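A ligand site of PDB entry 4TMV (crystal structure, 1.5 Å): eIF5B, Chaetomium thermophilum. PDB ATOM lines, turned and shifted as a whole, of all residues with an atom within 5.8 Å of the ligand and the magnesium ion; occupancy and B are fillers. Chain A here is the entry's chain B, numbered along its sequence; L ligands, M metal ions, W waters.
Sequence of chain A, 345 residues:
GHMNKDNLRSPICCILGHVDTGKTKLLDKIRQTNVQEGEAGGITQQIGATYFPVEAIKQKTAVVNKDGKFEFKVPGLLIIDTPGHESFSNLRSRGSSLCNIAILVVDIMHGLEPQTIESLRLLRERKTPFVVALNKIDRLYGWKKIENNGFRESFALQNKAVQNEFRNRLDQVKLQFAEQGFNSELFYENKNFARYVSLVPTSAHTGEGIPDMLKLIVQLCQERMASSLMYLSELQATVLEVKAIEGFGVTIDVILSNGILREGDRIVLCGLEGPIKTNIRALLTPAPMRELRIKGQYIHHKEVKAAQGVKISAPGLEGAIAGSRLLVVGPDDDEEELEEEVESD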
ATOM      1  N   GLY A  17       9.002  24.943 -10.649  1.00  0.00           N
ATOM      2  CA  GLY A  17       9.130  26.081 -11.554  1.00  0.00           C
ATOM      3  C   GLY A  17       8.002  27.068 -11.399  1.00  0.00           C
ATOM      4  O   GLY A  17       7.001  26.758 -10.749  1.00  0.00           O
ATOM      5  N   HIS A  18       8.139  28.221 -12.034  1.00  0.00           N
ATOM      6  CA  HIS A  18       7.194  29.318 -11.914  1.00  0.00           C
ATOM      7  C   HIS A  18       5.870  28.936 -12.555  1.00  0.00           C
ATOM      8  O   HIS A  18       5.790  27.979 -13.320  1.00  0.00           O
ATOM      9  CB  HIS A  18       7.778  30.566 -12.581  1.00  0.00           C
ATOM     10  CG  HIS A  18       7.098  31.844 -12.192  1.00  0.00           C
ATOM     11  ND1 HIS A  18       7.309  32.469 -10.985  1.00  0.00           N
ATOM     12  CD2 HIS A  18       6.238  32.632 -12.877  1.00  0.00           C
ATOM     13  CE1 HIS A  18       6.595  33.576 -10.940  1.00  0.00           C
ATOM     14  NE2 HIS A  18       5.931  33.700 -12.069  1.00  0.00           N
ATOM     15  N   VAL A  19       4.829  29.664 -12.214  1.00  0.00           N
ATOM     16  CA  VAL A  19       3.515  29.352 -12.716  1.00  0.00           C
ATOM     17  C   VAL A  19       3.504  29.368 -14.238  1.00  0.00           C
ATOM     18  O   VAL A  19       4.129  30.218 -14.867  1.00  0.00           O
ATOM     19  CB  VAL A  19       2.478  30.344 -12.154  1.00  0.00           C
ATOM     20  CG1 VAL A  19       2.710  31.737 -12.714  1.00  0.00           C
ATOM     21  CG2 VAL A  19       1.064  29.887 -12.439  1.00  0.00           C
ATOM     22  N   ASP A  20       2.828  28.382 -14.806  1.00  0.00           N
ATOM     23  CA  ASP A  20       2.565  28.272 -16.243  1.00  0.00           C
ATOM     24  C   ASP A  20       3.804  28.055 -17.116  1.00  0.00           C
ATOM     25  O   ASP A  20       3.783  28.315 -18.304  1.00  0.00           O
ATOM     26  CB  ASP A  20       1.756  29.460 -16.740  1.00  0.00           C
ATOM     27  CG  ASP A  20       0.259  29.261 -16.558  1.00  0.00           C
ATOM     28  OD1 ASP A  20      -0.473  30.262 -16.609  1.00  0.00           O
ATOM     29  OD2 ASP A  20      -0.199  28.111 -16.362  1.00  0.00           O
ATOM     30  N   THR A  21       4.882  27.551 -16.516  1.00  0.00           N
ATOM     31  CA  THR A  21       6.105  27.305 -17.266  1.00  0.00           C
ATOM     32  C   THR A  21       6.079  26.012 -18.098  1.00  0.00           C
ATOM     33  O   THR A  21       6.927  25.811 -18.947  1.00  0.00           O
ATOM     34  CB  THR A  21       7.344  27.347 -16.360  1.00  0.00           C
ATOM     35  OG1 THR A  21       7.128  26.496 -15.237  1.00  0.00           O
ATOM     36  CG2 THR A  21       7.589  28.758 -15.880  1.00  0.00           C
ATOM     37  N   GLY A  22       5.070  25.179 -17.859  1.00  0.00           N
ATOM     38  CA  GLY A  22       4.959  23.918 -18.564  1.00  0.00           C
ATOM     39  C   GLY A  22       5.276  22.621 -17.838  1.00  0.00           C
ATOM     40  O   GLY A  22       5.469  21.594 -18.476  1.00  0.00           O
ATOM     41  N   LYS A  23       5.359  22.654 -16.516  1.00  0.00           N
ATOM     42  CA  LYS A  23       5.712  21.445 -15.792  1.00  0.00           C
ATOM     43  C   LYS A  23       4.729  20.304 -16.016  1.00  0.00           C
ATOM     44  O   LYS A  23       5.121  19.192 -16.309  1.00  0.00           O
ATOM     45  CB  LYS A  23       5.737  21.726 -14.282  1.00  0.00           C
ATOM     46  CG  LYS A  23       6.580  22.909 -13.845  1.00  0.00           C
ATOM     47  CD  LYS A  23       6.443  23.190 -12.364  1.00  0.00           C
ATOM     48  CE  LYS A  23       5.115  23.847 -12.029  1.00  0.00           C
ATOM     49  NZ  LYS A  23       5.049  25.248 -12.519  1.00  0.00           N
ATOM     50  N   THR A  24       3.433  20.592 -15.905  1.00  0.00           N
ATOM     51  CA  THR A  24       2.432  19.578 -16.154  1.00  0.00           C
ATOM     52  C   THR A  24       2.391  19.146 -17.619  1.00  0.00           C
ATOM     53  O   THR A  24       2.247  17.978 -17.926  1.00  0.00           O
ATOM     54  CB  THR A  24       1.050  20.021 -15.657  1.00  0.00           C
ATOM     55  OG1 THR A  24       1.135  20.329 -14.265  1.00  0.00           O
ATOM     56  CG2 THR A  24       0.031  18.908 -15.853  1.00  0.00           C
ATOM     57  N   LYS A  25       2.528  20.124 -18.511  1.00  0.00           N
ATOM     58  CA  LYS A  25       2.515  19.822 -19.951  1.00  0.00           C
ATOM     59  C   LYS A  25       3.704  18.930 -20.334  1.00  0.00           C
ATOM     60  O   LYS A  25       3.528  18.036 -21.203  1.00  0.00           O
ATOM     61  CB  LYS A  25       2.509  21.113 -20.754  1.00  0.00           C
ATOM     62  CG  LYS A  25       1.958  20.955 -22.178  1.00  0.00           C
ATOM     63  CD  LYS A  25       0.407  20.841 -22.138  1.00  0.00           C
ATOM     64  CE  LYS A  25      -0.037  20.776 -23.613  1.00  0.00           C
ATOM     65  NZ  LYS A  25      -1.489  20.528 -23.647  1.00  0.00           N
ATOM     66  N   LEU A  26       4.872  19.204 -19.767  1.00  0.00           N
ATOM     67  CA  LEU A  26       6.002  18.296 -20.032  1.00  0.00           C
ATOM     68  C   LEU A  26       5.633  16.875 -19.585  1.00  0.00           C
ATOM     69  O   LEU A  26       5.869  15.906 -20.318  1.00  0.00           O
ATOM     70  CB  LEU A  26       7.263  18.738 -19.312  1.00  0.00           C
ATOM     71  CG  LEU A  26       7.981  19.947 -19.906  1.00  0.00           C
ATOM     72  CD1 LEU A  26       8.957  20.556 -18.916  1.00  0.00           C
ATOM     73  CD2 LEU A  26       8.729  19.537 -21.228  1.00  0.00           C
ATOM     74  N   GLN A  36      -3.273  18.354 -17.977  1.00  0.00           N
ATOM     75  CA  GLN A  36      -3.287  19.814 -17.895  1.00  0.00           C
ATOM     76  C   GLN A  36      -4.644  20.411 -18.348  1.00  0.00           C
ATOM     77  O   GLN A  36      -5.156  21.351 -17.706  1.00  0.00           O
ATOM     78  CB  GLN A  36      -2.136  20.384 -18.730  1.00  0.00           C
ATOM     79  CG  GLN A  36      -1.802  21.811 -18.325  1.00  0.00           C
ATOM     80  CD  GLN A  36      -2.649  22.858 -19.084  1.00  0.00           C
ATOM     81  OE1 GLN A  36      -3.298  22.528 -20.097  1.00  0.00           O
ATOM     82  NE2 GLN A  36      -2.649  24.094 -18.600  1.00  0.00           N
ATOM     83  N   GLU A  39      -7.360  20.311 -15.612  1.00  0.00           N
ATOM     84  CA  GLU A  39      -7.232  21.154 -14.427  1.00  0.00           C
ATOM     85  C   GLU A  39      -8.091  22.403 -14.519  1.00  0.00           C
ATOM     86  O   GLU A  39      -8.102  23.075 -15.534  1.00  0.00           O
ATOM     87  CB  GLU A  39      -5.774  21.569 -14.209  1.00  0.00           C
ATOM     88  CG  GLU A  39      -4.832  20.426 -13.868  1.00  0.00           C
ATOM     89  CD  GLU A  39      -3.398  20.894 -13.769  1.00  0.00           C
ATOM     90  OE1 GLU A  39      -3.038  21.852 -14.481  1.00  0.00           O
ATOM     91  OE2 GLU A  39      -2.642  20.306 -12.974  1.00  0.00           O
ATOM     92  N   GLY A  42      -6.419  25.540 -15.596  1.00  0.00           N
ATOM     93  CA  GLY A  42      -5.123  25.052 -16.006  1.00  0.00           C
ATOM     94  C   GLY A  42      -4.093  25.216 -14.895  1.00  0.00           C
ATOM     95  O   GLY A  42      -2.912  25.359 -15.160  1.00  0.00           O
ATOM     96  N   ILE A  43      -4.542  25.145 -13.659  1.00  0.00           N
ATOM     97  CA  ILE A  43      -3.688  25.354 -12.510  1.00  0.00           C
ATOM     98  C   ILE A  43      -3.528  24.069 -11.714  1.00  0.00           C
ATOM     99  O   ILE A  43      -4.498  23.433 -11.343  1.00  0.00           O
ATOM    100  CB  ILE A  43      -4.271  26.412 -11.559  1.00  0.00           C
ATOM    101  CG1 ILE A  43      -4.502  27.733 -12.297  1.00  0.00           C
ATOM    102  CG2 ILE A  43      -3.383  26.604 -10.343  1.00  0.00           C
ATOM    103  CD1 ILE A  43      -3.248  28.498 -12.602  1.00  0.00           C
ATOM    104  N   THR A  44      -2.283  23.686 -11.444  1.00  0.00           N
ATOM    105  CA  THR A  44      -2.043  22.521 -10.614  1.00  0.00           C
ATOM    106  C   THR A  44      -2.195  22.959  -9.158  1.00  0.00           C
ATOM    107  O   THR A  44      -1.568  23.927  -8.746  1.00  0.00           O
ATOM    108  CB  THR A  44      -0.629  21.961 -10.858  1.00  0.00           C
ATOM    109  OG1 THR A  44      -0.525  21.527 -12.215  1.00  0.00           O
ATOM    110  CG2 THR A  44      -0.351  20.792  -9.951  1.00  0.00           C
ATOM    111  N   ASP A  81       4.920  16.075  -9.666  1.00  0.00           N
ATOM    112  CA  ASP A  81       4.549  17.371 -10.242  1.00  0.00           C
ATOM    113  C   ASP A  81       4.145  18.283  -9.067  1.00  0.00           C
ATOM    114  O   ASP A  81       3.601  17.776  -8.086  1.00  0.00           O
ATOM    115  CB  ASP A  81       3.366  17.168 -11.204  1.00  0.00           C
ATOM    116  CG  ASP A  81       3.105  18.346 -12.073  1.00  0.00           C
ATOM    117  OD1 ASP A  81       3.852  19.349 -12.046  1.00  0.00           O
ATOM    118  OD2 ASP A  81       2.008  18.262 -12.775  1.00  0.00           O
ATOM    119  N   THR A  82       4.492  19.542  -9.139  1.00  0.00           N
ATOM    120  CA  THR A  82       4.182  20.488  -8.069  1.00  0.00           C
ATOM    121  C   THR A  82       3.561  21.731  -8.638  1.00  0.00           C
ATOM    122  O   THR A  82       3.764  22.082  -9.812  1.00  0.00           O
ATOM    123  CB  THR A  82       5.465  20.931  -7.287  1.00  0.00           C
ATOM    124  OG1 THR A  82       6.398  21.608  -8.187  1.00  0.00           O
ATOM    125  CG2 THR A  82       6.133  19.724  -6.660  1.00  0.00           C
ATOM    126  N   PRO A  83       2.797  22.444  -7.820  1.00  0.00           N
ATOM    127  CA  PRO A  83       2.235  23.715  -8.241  1.00  0.00           C
ATOM    128  C   PRO A  83       3.243  24.785  -8.377  1.00  0.00           C
ATOM    129  O   PRO A  83       4.143  24.893  -7.536  1.00  0.00           O
ATOM    130  CB  PRO A  83       1.262  24.104  -7.097  1.00  0.00           C
ATOM    131  CG  PRO A  83       1.011  22.858  -6.391  1.00  0.00           C
ATOM    132  CD  PRO A  83       2.282  21.971  -6.520  1.00  0.00           C
ATOM    133  N   GLY A  84       3.122  25.620  -9.399  1.00  0.00           N
ATOM    134  CA  GLY A  84       3.922  26.842  -9.504  1.00  0.00           C
ATOM    135  C   GLY A  84       3.268  28.102  -8.965  1.00  0.00           C
ATOM    136  O   GLY A  84       3.914  29.117  -8.783  1.00  0.00           O
ATOM    137  N   HIS A  85       1.929  28.058  -8.743  1.00  0.00           N
ATOM    138  CA  HIS A  85       1.267  29.271  -8.333  1.00  0.00           C
ATOM    139  C   HIS A  85       1.835  29.790  -6.998  1.00  0.00           C
ATOM    140  O   HIS A  85       2.122  28.989  -6.098  1.00  0.00           O
ATOM    141  CB  HIS A  85      -0.264  29.002  -8.255  1.00  0.00           C
ATOM    142  CG  HIS A  85      -1.043  30.213  -7.941  1.00  0.00           C
ATOM    143  ND1 HIS A  85      -1.260  30.671  -6.649  1.00  0.00           N
ATOM    144  CD2 HIS A  85      -1.733  31.067  -8.748  1.00  0.00           C
ATOM    145  CE1 HIS A  85      -1.953  31.794  -6.672  1.00  0.00           C
ATOM    146  NE2 HIS A  85      -2.311  32.017  -7.928  1.00  0.00           N
ATOM    147  N   ASN A 135      12.141  25.465 -21.297  1.00  0.00           N
ATOM    148  CA  ASN A 135      10.921  25.075 -21.983  1.00  0.00           C
ATOM    149  C   ASN A 135      10.368  26.104 -22.975  1.00  0.00           C
ATOM    150  O   ASN A 135      10.692  27.274 -22.900  1.00  0.00           O
ATOM    151  CB  ASN A 135       9.843  24.660 -20.992  1.00  0.00           C
ATOM    152  CG  ASN A 135       8.746  23.827 -21.629  1.00  0.00           C
ATOM    153  OD1 ASN A 135       9.011  23.019 -22.510  1.00  0.00           O
ATOM    154  ND2 ASN A 135       7.525  24.044 -21.198  1.00  0.00           N
ATOM    155  N   LYS A 136       9.481  25.627 -23.842  1.00  0.00           N
ATOM    156  CA  LYS A 136       8.795  26.447 -24.849  1.00  0.00           C
ATOM    157  C   LYS A 136       9.654  26.956 -26.013  1.00  0.00           C
ATOM    158  O   LYS A 136       9.417  28.038 -26.526  1.00  0.00           O
ATOM    159  CB  LYS A 136       8.060  27.627 -24.186  1.00  0.00           C
ATOM    160  CG  LYS A 136       7.218  27.218 -22.979  1.00  0.00           C
ATOM    161  CD  LYS A 136       6.116  28.225 -22.699  1.00  0.00           C
ATOM    162  CE  LYS A 136       5.346  27.856 -21.446  1.00  0.00           C
ATOM    163  NZ  LYS A 136       4.320  28.882 -21.117  1.00  0.00           N
ATOM    164  N   ILE A 137      10.625  26.156 -26.418  1.00  0.00           N
ATOM    165  CA  ILE A 137      11.494  26.530 -27.527  1.00  0.00           C
ATOM    166  C   ILE A 137      10.698  26.692 -28.825  1.00  0.00           C
ATOM    167  O   ILE A 137      11.135  27.382 -29.739  1.00  0.00           O
ATOM    168  CB  ILE A 137      12.675  25.565 -27.749  1.00  0.00           C
ATOM    169  CG1 ILE A 137      12.202  24.159 -28.110  1.00  0.00           C
ATOM    170  CG2 ILE A 137      13.588  25.546 -26.533  1.00  0.00           C
ATOM    171  CD1 ILE A 137      13.334  23.171 -28.274  1.00  0.00           C
ATOM    172  N   ASP A 138       9.541  26.038 -28.918  1.00  0.00           N
ATOM    173  CA  ASP A 138       8.732  26.157 -30.122  1.00  0.00           C
ATOM    174  C   ASP A 138       8.213  27.616 -30.324  1.00  0.00           C
ATOM    175  O   ASP A 138       7.656  27.950 -31.394  1.00  0.00           O
ATOM    176  CB  ASP A 138       7.605  25.150 -30.055  1.00  0.00           C
ATOM    177  CG  ASP A 138       6.694  25.426 -28.924  1.00  0.00           C
ATOM    178  OD1 ASP A 138       5.629  26.060 -29.153  1.00  0.00           O
ATOM    179  OD2 ASP A 138       7.042  25.072 -27.803  1.00  0.00           O
ATOM    180  N   ARG A 139       8.344  28.460 -29.299  1.00  0.00           N
ATOM    181  CA  ARG A 139       7.947  29.873 -29.389  1.00  0.00           C
ATOM    182  C   ARG A 139       9.025  30.760 -30.033  1.00  0.00           C
ATOM    183  O   ARG A 139       8.800  31.931 -30.334  1.00  0.00           O
ATOM    184  CB  ARG A 139       7.605  30.412 -28.008  1.00  0.00           C
ATOM    185  CG  ARG A 139       6.356  29.786 -27.410  1.00  0.00           C
ATOM    186  CD  ARG A 139       5.217  30.798 -27.454  1.00  0.00           C
ATOM    187  NE  ARG A 139       5.309  31.645 -26.261  1.00  0.00           N
ATOM    188  CZ  ARG A 139       5.676  32.928 -26.252  1.00  0.00           C
ATOM    189  NH1 ARG A 139       5.760  33.584 -25.105  1.00  0.00           N
ATOM    190  NH2 ARG A 139       5.958  33.553 -27.391  1.00  0.00           N
ATOM    191  N   THR A 202      13.666  22.468 -24.233  1.00  0.00           N
ATOM    192  CA  THR A 202      12.574  21.546 -24.435  1.00  0.00           C
ATOM    193  C   THR A 202      11.364  22.265 -25.011  1.00  0.00           C
ATOM    194  O   THR A 202      11.267  23.475 -24.935  1.00  0.00           O
ATOM    195  CB  THR A 202      12.066  20.872 -23.121  1.00  0.00           C
ATOM    196  OG1 THR A 202      11.650  21.856 -22.168  1.00  0.00           O
ATOM    197  CG2 THR A 202      13.233  20.038 -22.416  1.00  0.00           C
ATOM    198  N   SER A 203      10.490  21.439 -25.577  1.00  0.00           N
ATOM    199  CA  SER A 203       9.133  21.913 -25.862  1.00  0.00           C
ATOM    200  C   SER A 203       8.195  20.834 -25.400  1.00  0.00           C
ATOM    201  O   SER A 203       8.232  19.715 -25.909  1.00  0.00           O
ATOM    202  CB  SER A 203       8.923  22.194 -27.355  1.00  0.00           C
ATOM    203  OG  SER A 203       7.510  22.449 -27.595  1.00  0.00           O
ATOM    204  N   ALA A 204       7.289  21.209 -24.465  1.00  0.00           N
ATOM    205  CA  ALA A 204       6.269  20.239 -24.083  1.00  0.00           C
ATOM    206  C   ALA A 204       5.240  20.066 -25.192  1.00  0.00           C
ATOM    207  O   ALA A 204       4.538  19.069 -25.225  1.00  0.00           O
ATOM    208  CB  ALA A 204       5.561  20.662 -22.789  1.00  0.00           C
ATOM    209  N   HIS A 205       5.175  21.048 -26.095  1.00  0.00           N
ATOM    210  CA  HIS A 205       4.190  20.936 -27.181  1.00  0.00           C
ATOM    211  C   HIS A 205       4.662  19.981 -28.307  1.00  0.00           C
ATOM    212  O   HIS A 205       3.924  19.100 -28.766  1.00  0.00           O
ATOM    213  CB  HIS A 205       3.872  22.328 -27.721  1.00  0.00           C
ATOM    214  CG  HIS A 205       2.868  23.066 -26.854  1.00  0.00           C
ATOM    215  ND1 HIS A 205       2.069  24.088 -27.306  1.00  0.00           N
ATOM    216  CD2 HIS A 205       2.516  22.856 -25.563  1.00  0.00           C
ATOM    217  CE1 HIS A 205       1.272  24.497 -26.333  1.00  0.00           C
ATOM    218  NE2 HIS A 205       1.491  23.735 -25.268  1.00  0.00           N
ATOM    219  N   THR A 206       5.924  20.113 -28.701  1.00  0.00           N
ATOM    220  CA  THR A 206       6.418  19.229 -29.781  1.00  0.00           C
ATOM    221  C   THR A 206       7.143  17.994 -29.291  1.00  0.00           C
ATOM    222  O   THR A 206       7.368  17.077 -30.084  1.00  0.00           O
ATOM    223  CB  THR A 206       7.442  19.980 -30.704  1.00  0.00           C
ATOM    224  OG1 THR A 206       8.648  20.222 -29.950  1.00  0.00           O
ATOM    225  CG2 THR A 206       6.947  21.363 -31.139  1.00  0.00           C
ATOM    226  N   ARG A 293      -2.753  11.762  -8.773  1.00  0.00           N
ATOM    227  CA  ARG A 293      -3.691  12.781  -8.293  1.00  0.00           C
ATOM    228  C   ARG A 293      -4.987  12.834  -9.098  1.00  0.00           C
ATOM    229  O   ARG A 293      -5.919  13.578  -8.707  1.00  0.00           O
ATOM    230  CB  ARG A 293      -3.063  14.189  -8.302  1.00  0.00           C
ATOM    231  CG  ARG A 293      -2.724  14.750  -9.714  1.00  0.00           C
ATOM    232  CD  ARG A 293      -2.020  16.048  -9.474  1.00  0.00           C
ATOM    233  NE  ARG A 293      -1.287  16.577 -10.632  1.00  0.00           N
ATOM    234  CZ  ARG A 293      -1.697  17.535 -11.406  1.00  0.00           C
ATOM    235  NH1 ARG A 293      -2.913  18.109 -11.238  1.00  0.00           N
ATOM    236  NH2 ARG A 293      -0.930  18.032 -12.367  1.00  0.00           N
HETATM  237  P1  LIG L   1       1.312  25.475 -12.915  1.00  0.00           P
HETATM  238  O1  LIG L   1       1.661  25.456 -14.483  1.00  0.00           O
HETATM  239  S1  LIG L   1      -0.228  26.659 -12.732  1.00  0.00           S
HETATM  240  O2  LIG L   1       0.978  24.009 -12.388  1.00  0.00           O
HETATM  241  O3  LIG L   1       2.560  26.057 -12.122  1.00  0.00           O
HETATM  242  P2  LIG L   1       2.621  24.416 -15.252  1.00  0.00           P
HETATM  243  O4  LIG L   1       4.047  24.774 -15.032  1.00  0.00           O
HETATM  244  O5  LIG L   1       2.190  23.030 -14.926  1.00  0.00           O
HETATM  245  P3  LIG L   1       1.147  24.078 -17.649  1.00  0.00           P
HETATM  246  O6  LIG L   1      -0.156  24.324 -16.950  1.00  0.00           O
HETATM  247  O7  LIG L   1       1.540  22.675 -17.978  1.00  0.00           O
HETATM  248  O8  LIG L   1       2.301  24.765 -16.780  1.00  0.00           O
HETATM  249  O9  LIG L   1       1.207  24.957 -18.991  1.00  0.00           O
HETATM  250  C1  LIG L   1       0.796  26.312 -18.944  1.00  0.00           C
HETATM  251  C2  LIG L   1       0.527  26.828 -20.356  1.00  0.00           C
HETATM  252  O10 LIG L   1       1.738  26.868 -21.094  1.00  0.00           O
HETATM  253  C3  LIG L   1      -0.414  25.907 -21.101  1.00  0.00           C
HETATM  254  O11 LIG L   1      -1.232  26.678 -21.983  1.00  0.00           O
HETATM  255  C4  LIG L   1       0.525  25.059 -21.932  1.00  0.00           C
HETATM  256  O12 LIG L   1      -0.104  24.559 -23.108  1.00  0.00           O
HETATM  257  C5  LIG L   1       1.611  26.070 -22.249  1.00  0.00           C
HETATM  258  N1  LIG L   1       2.876  25.376 -22.541  1.00  0.00           N
HETATM  259  C6  LIG L   1       3.509  24.501 -21.743  1.00  0.00           C
HETATM  260  N2  LIG L   1       4.642  24.055 -22.332  1.00  0.00           N
HETATM  261  C7  LIG L   1       4.720  24.658 -23.524  1.00  0.00           C
HETATM  262  C8  LIG L   1       5.662  24.643 -24.658  1.00  0.00           C
HETATM  263  O13 LIG L   1       6.685  23.946 -24.634  1.00  0.00           O
HETATM  264  N3  LIG L   1       5.380  25.416 -25.705  1.00  0.00           N
HETATM  265  C9  LIG L   1       4.286  26.189 -25.760  1.00  0.00           C
HETATM  266  N4  LIG L   1       4.086  26.939 -26.871  1.00  0.00           N
HETATM  267  N5  LIG L   1       3.383  26.256 -24.764  1.00  0.00           N
HETATM  268  C10 LIG L   1       3.557  25.523 -23.653  1.00  0.00           C
HETATM  269 MG    MG M   1       0.981  22.324 -13.454  1.00  0.00          MG
HETATM  270  O   HOH W   1      -0.592  22.717 -14.841  1.00  0.00           O
HETATM  271  O   HOH W   2       2.548  21.692 -12.174  1.00  0.00           O
HETATM  272  O   HOH W   3      -2.562  23.208 -22.778  1.00  0.00           O
HETATM  273  O   HOH W   4       0.050  26.046  -9.624  1.00  0.00           O
HETATM  274  O   HOH W   5      -1.216  26.392 -25.090  1.00  0.00           O
HETATM  275  O   HOH W   6       0.280  29.337 -22.803  1.00  0.00           O
HETATM  276  O   HOH W   7       1.803  28.596 -27.355  1.00  0.00           O
HETATM  277  O   HOH W   8       2.763  29.028 -23.701  1.00  0.00           O
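O10 of the ligand sits at hydrogen-bond distance from NZ of Lys 136. O6 of the ligand is in hydrogen-bond range of NE2 of Gln 36, at 3.0 Å. An oxygen (O4) of the ligand is in salt-bridge range of the side-chain amino group of Lys 23 (2.7 Å). The side-chain carboxylate (OD2) of Asp 138 lies within hydrogen-bond range of a nitrogen (N3) of the ligand (2.7 Å). The backbone NH of Gly 84 sits at hydrogen-bond distance from an oxygen (O3) of the ligand (2.8 Å). The backbone NH (N) of Ala 204 lies within hydrogen-bond range of an oxygen (O13) of the ligand (2.8 Å). An oxygen (O12) of the ligand lies within hydrogen-bond range of a ring nitrogen (NE2) of His 205 (2.8 Å). The backbone NH (N) of Thr 44 lies close to an oxygen (O2) of the ligand, at 3.4 Å. An oxygen (O8) of the ligand lies within hydrogen-bond range of the backbone NH (N) of Gly 22 (3.0 Å). N2 of the ligand is in hydrogen-bond range of ND2 of Asn 135. O13 of the ligand sits close to OG of Ser 203 (3.4 Å). N of Thr 21 is in hydrogen-bond range of O4 of the ligand, 3.3 Å away. The backbone NH (N) of Lys 25 sits at hydrogen-bond distance from an oxygen (O7) of the ligand, 2.8 Å away. O4 of the ligand sits at hydrogen-bond distance from N of Lys 23. An oxygen (O1) of the ligand lies within hydrogen-bond range of the backbone NH of Asp 20, 3.2 Å away. An oxygen (O13) of the ligand lies close to the backbone NH of Lys 136 (3.4 Å). The backbone NH (N) of Thr 24 sits at hydrogen-bond distance from an oxygen (O7) of the ligand.
The backbone carbonyl oxygen (O) of Asp 20 lies within hydrogen-bond range of the side-chain amino group (NZ) of Lys 136, at 2.9 Å. The side-chain carboxylate (OD2) of Asp 138 lies within hydrogen-bond range of the side-chain hydroxyl (OG) of Ser 203 (2.7 Å). The side-chain amide oxygen (OD1) of Asn 135 sits at hydrogen-bond distance from the side-chain hydroxyl (OG1) of Thr 202 (2.9 Å). The backbone carbonyl oxygen (O) of Thr 202 is in hydrogen-bond range of the backbone NH (N) of Lys 136 (3.0 Å). O of His 18 sits at hydrogen-bond distance from OG1 of Thr 21. NZ of Lys 23 sits at hydrogen-bond distance from O of Gly 17 (3.0 Å). OE2 of Glu 39 sits close to OG1 of Thr 44. N of His 205 lies close to OG of Ser 203 (3.1 Å).
Water W2 lies within hydrogen-bond range of OD1 of Asp 81 (2.7 Å) and O of Thr 82 (2.7 Å). Water W1 lies within hydrogen-bond range of OE1 of Glu 39 (2.6 Å) and O6 of the ligand (2.7 Å). Water W3 lies within hydrogen-bond range of O12 of the ligand (2.8 Å), OE1 of Gln 36 (2.9 Å) and NZ of Lys 25 (3.0 Å). Water W8 bridges NZ of Lys 136 (3.0 Å) and N5 of the ligand (3.0 Å). Water W4 lies within hydrogen-bond range of the backbone carbonyl oxygen of Thr 44 (2.8 Å), the backbone NH of His 85 (2.9 Å), the backbone NH of Gly 84 (3.1 Å) and a sulfur (S1) of the ligand (3.2 Å).
O of Gly 42 lies close to O6 of the ligand, 3.4 Å away. His 18 touches the ligand (O to O3, 3.9 Å). CA of Val 19 touches O3 of the ligand, at 3.5 Å. Ile 43 touches the ligand (CD1 to S1, 3.5 Å). His 85 touches the ligand. Arg 139 touches the ligand (CG to N4, 3.7 Å). Hydrophobic or aromatic side chains that line the ligand: Val 19, Ile 43, Ala 204 and His 205. Of the 31 residues printed, 21 come within 4 Å of the ligand. The nearest printed residue that does not touch the ligand is Pro 83 (4.01 Å).
An oxygen (O2) of the ligand is bound to the magnesium ion (2.0 Å). O5 of the ligand is bound to the magnesium ion (2.0 Å). The magnesium ion is bound by the side-chain hydroxyl (OG1) of Thr 44. The magnesium ion is bound by water W2 (2.1 Å). Water W1 binds the magnesium ion (2.1 Å). The side-chain hydroxyl (OG1) of Thr 24 binds the magnesium ion (2.2 Å).
Two residues have an atom within 4 Å of the magnesium ion: Thr 24 and Thr 44.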
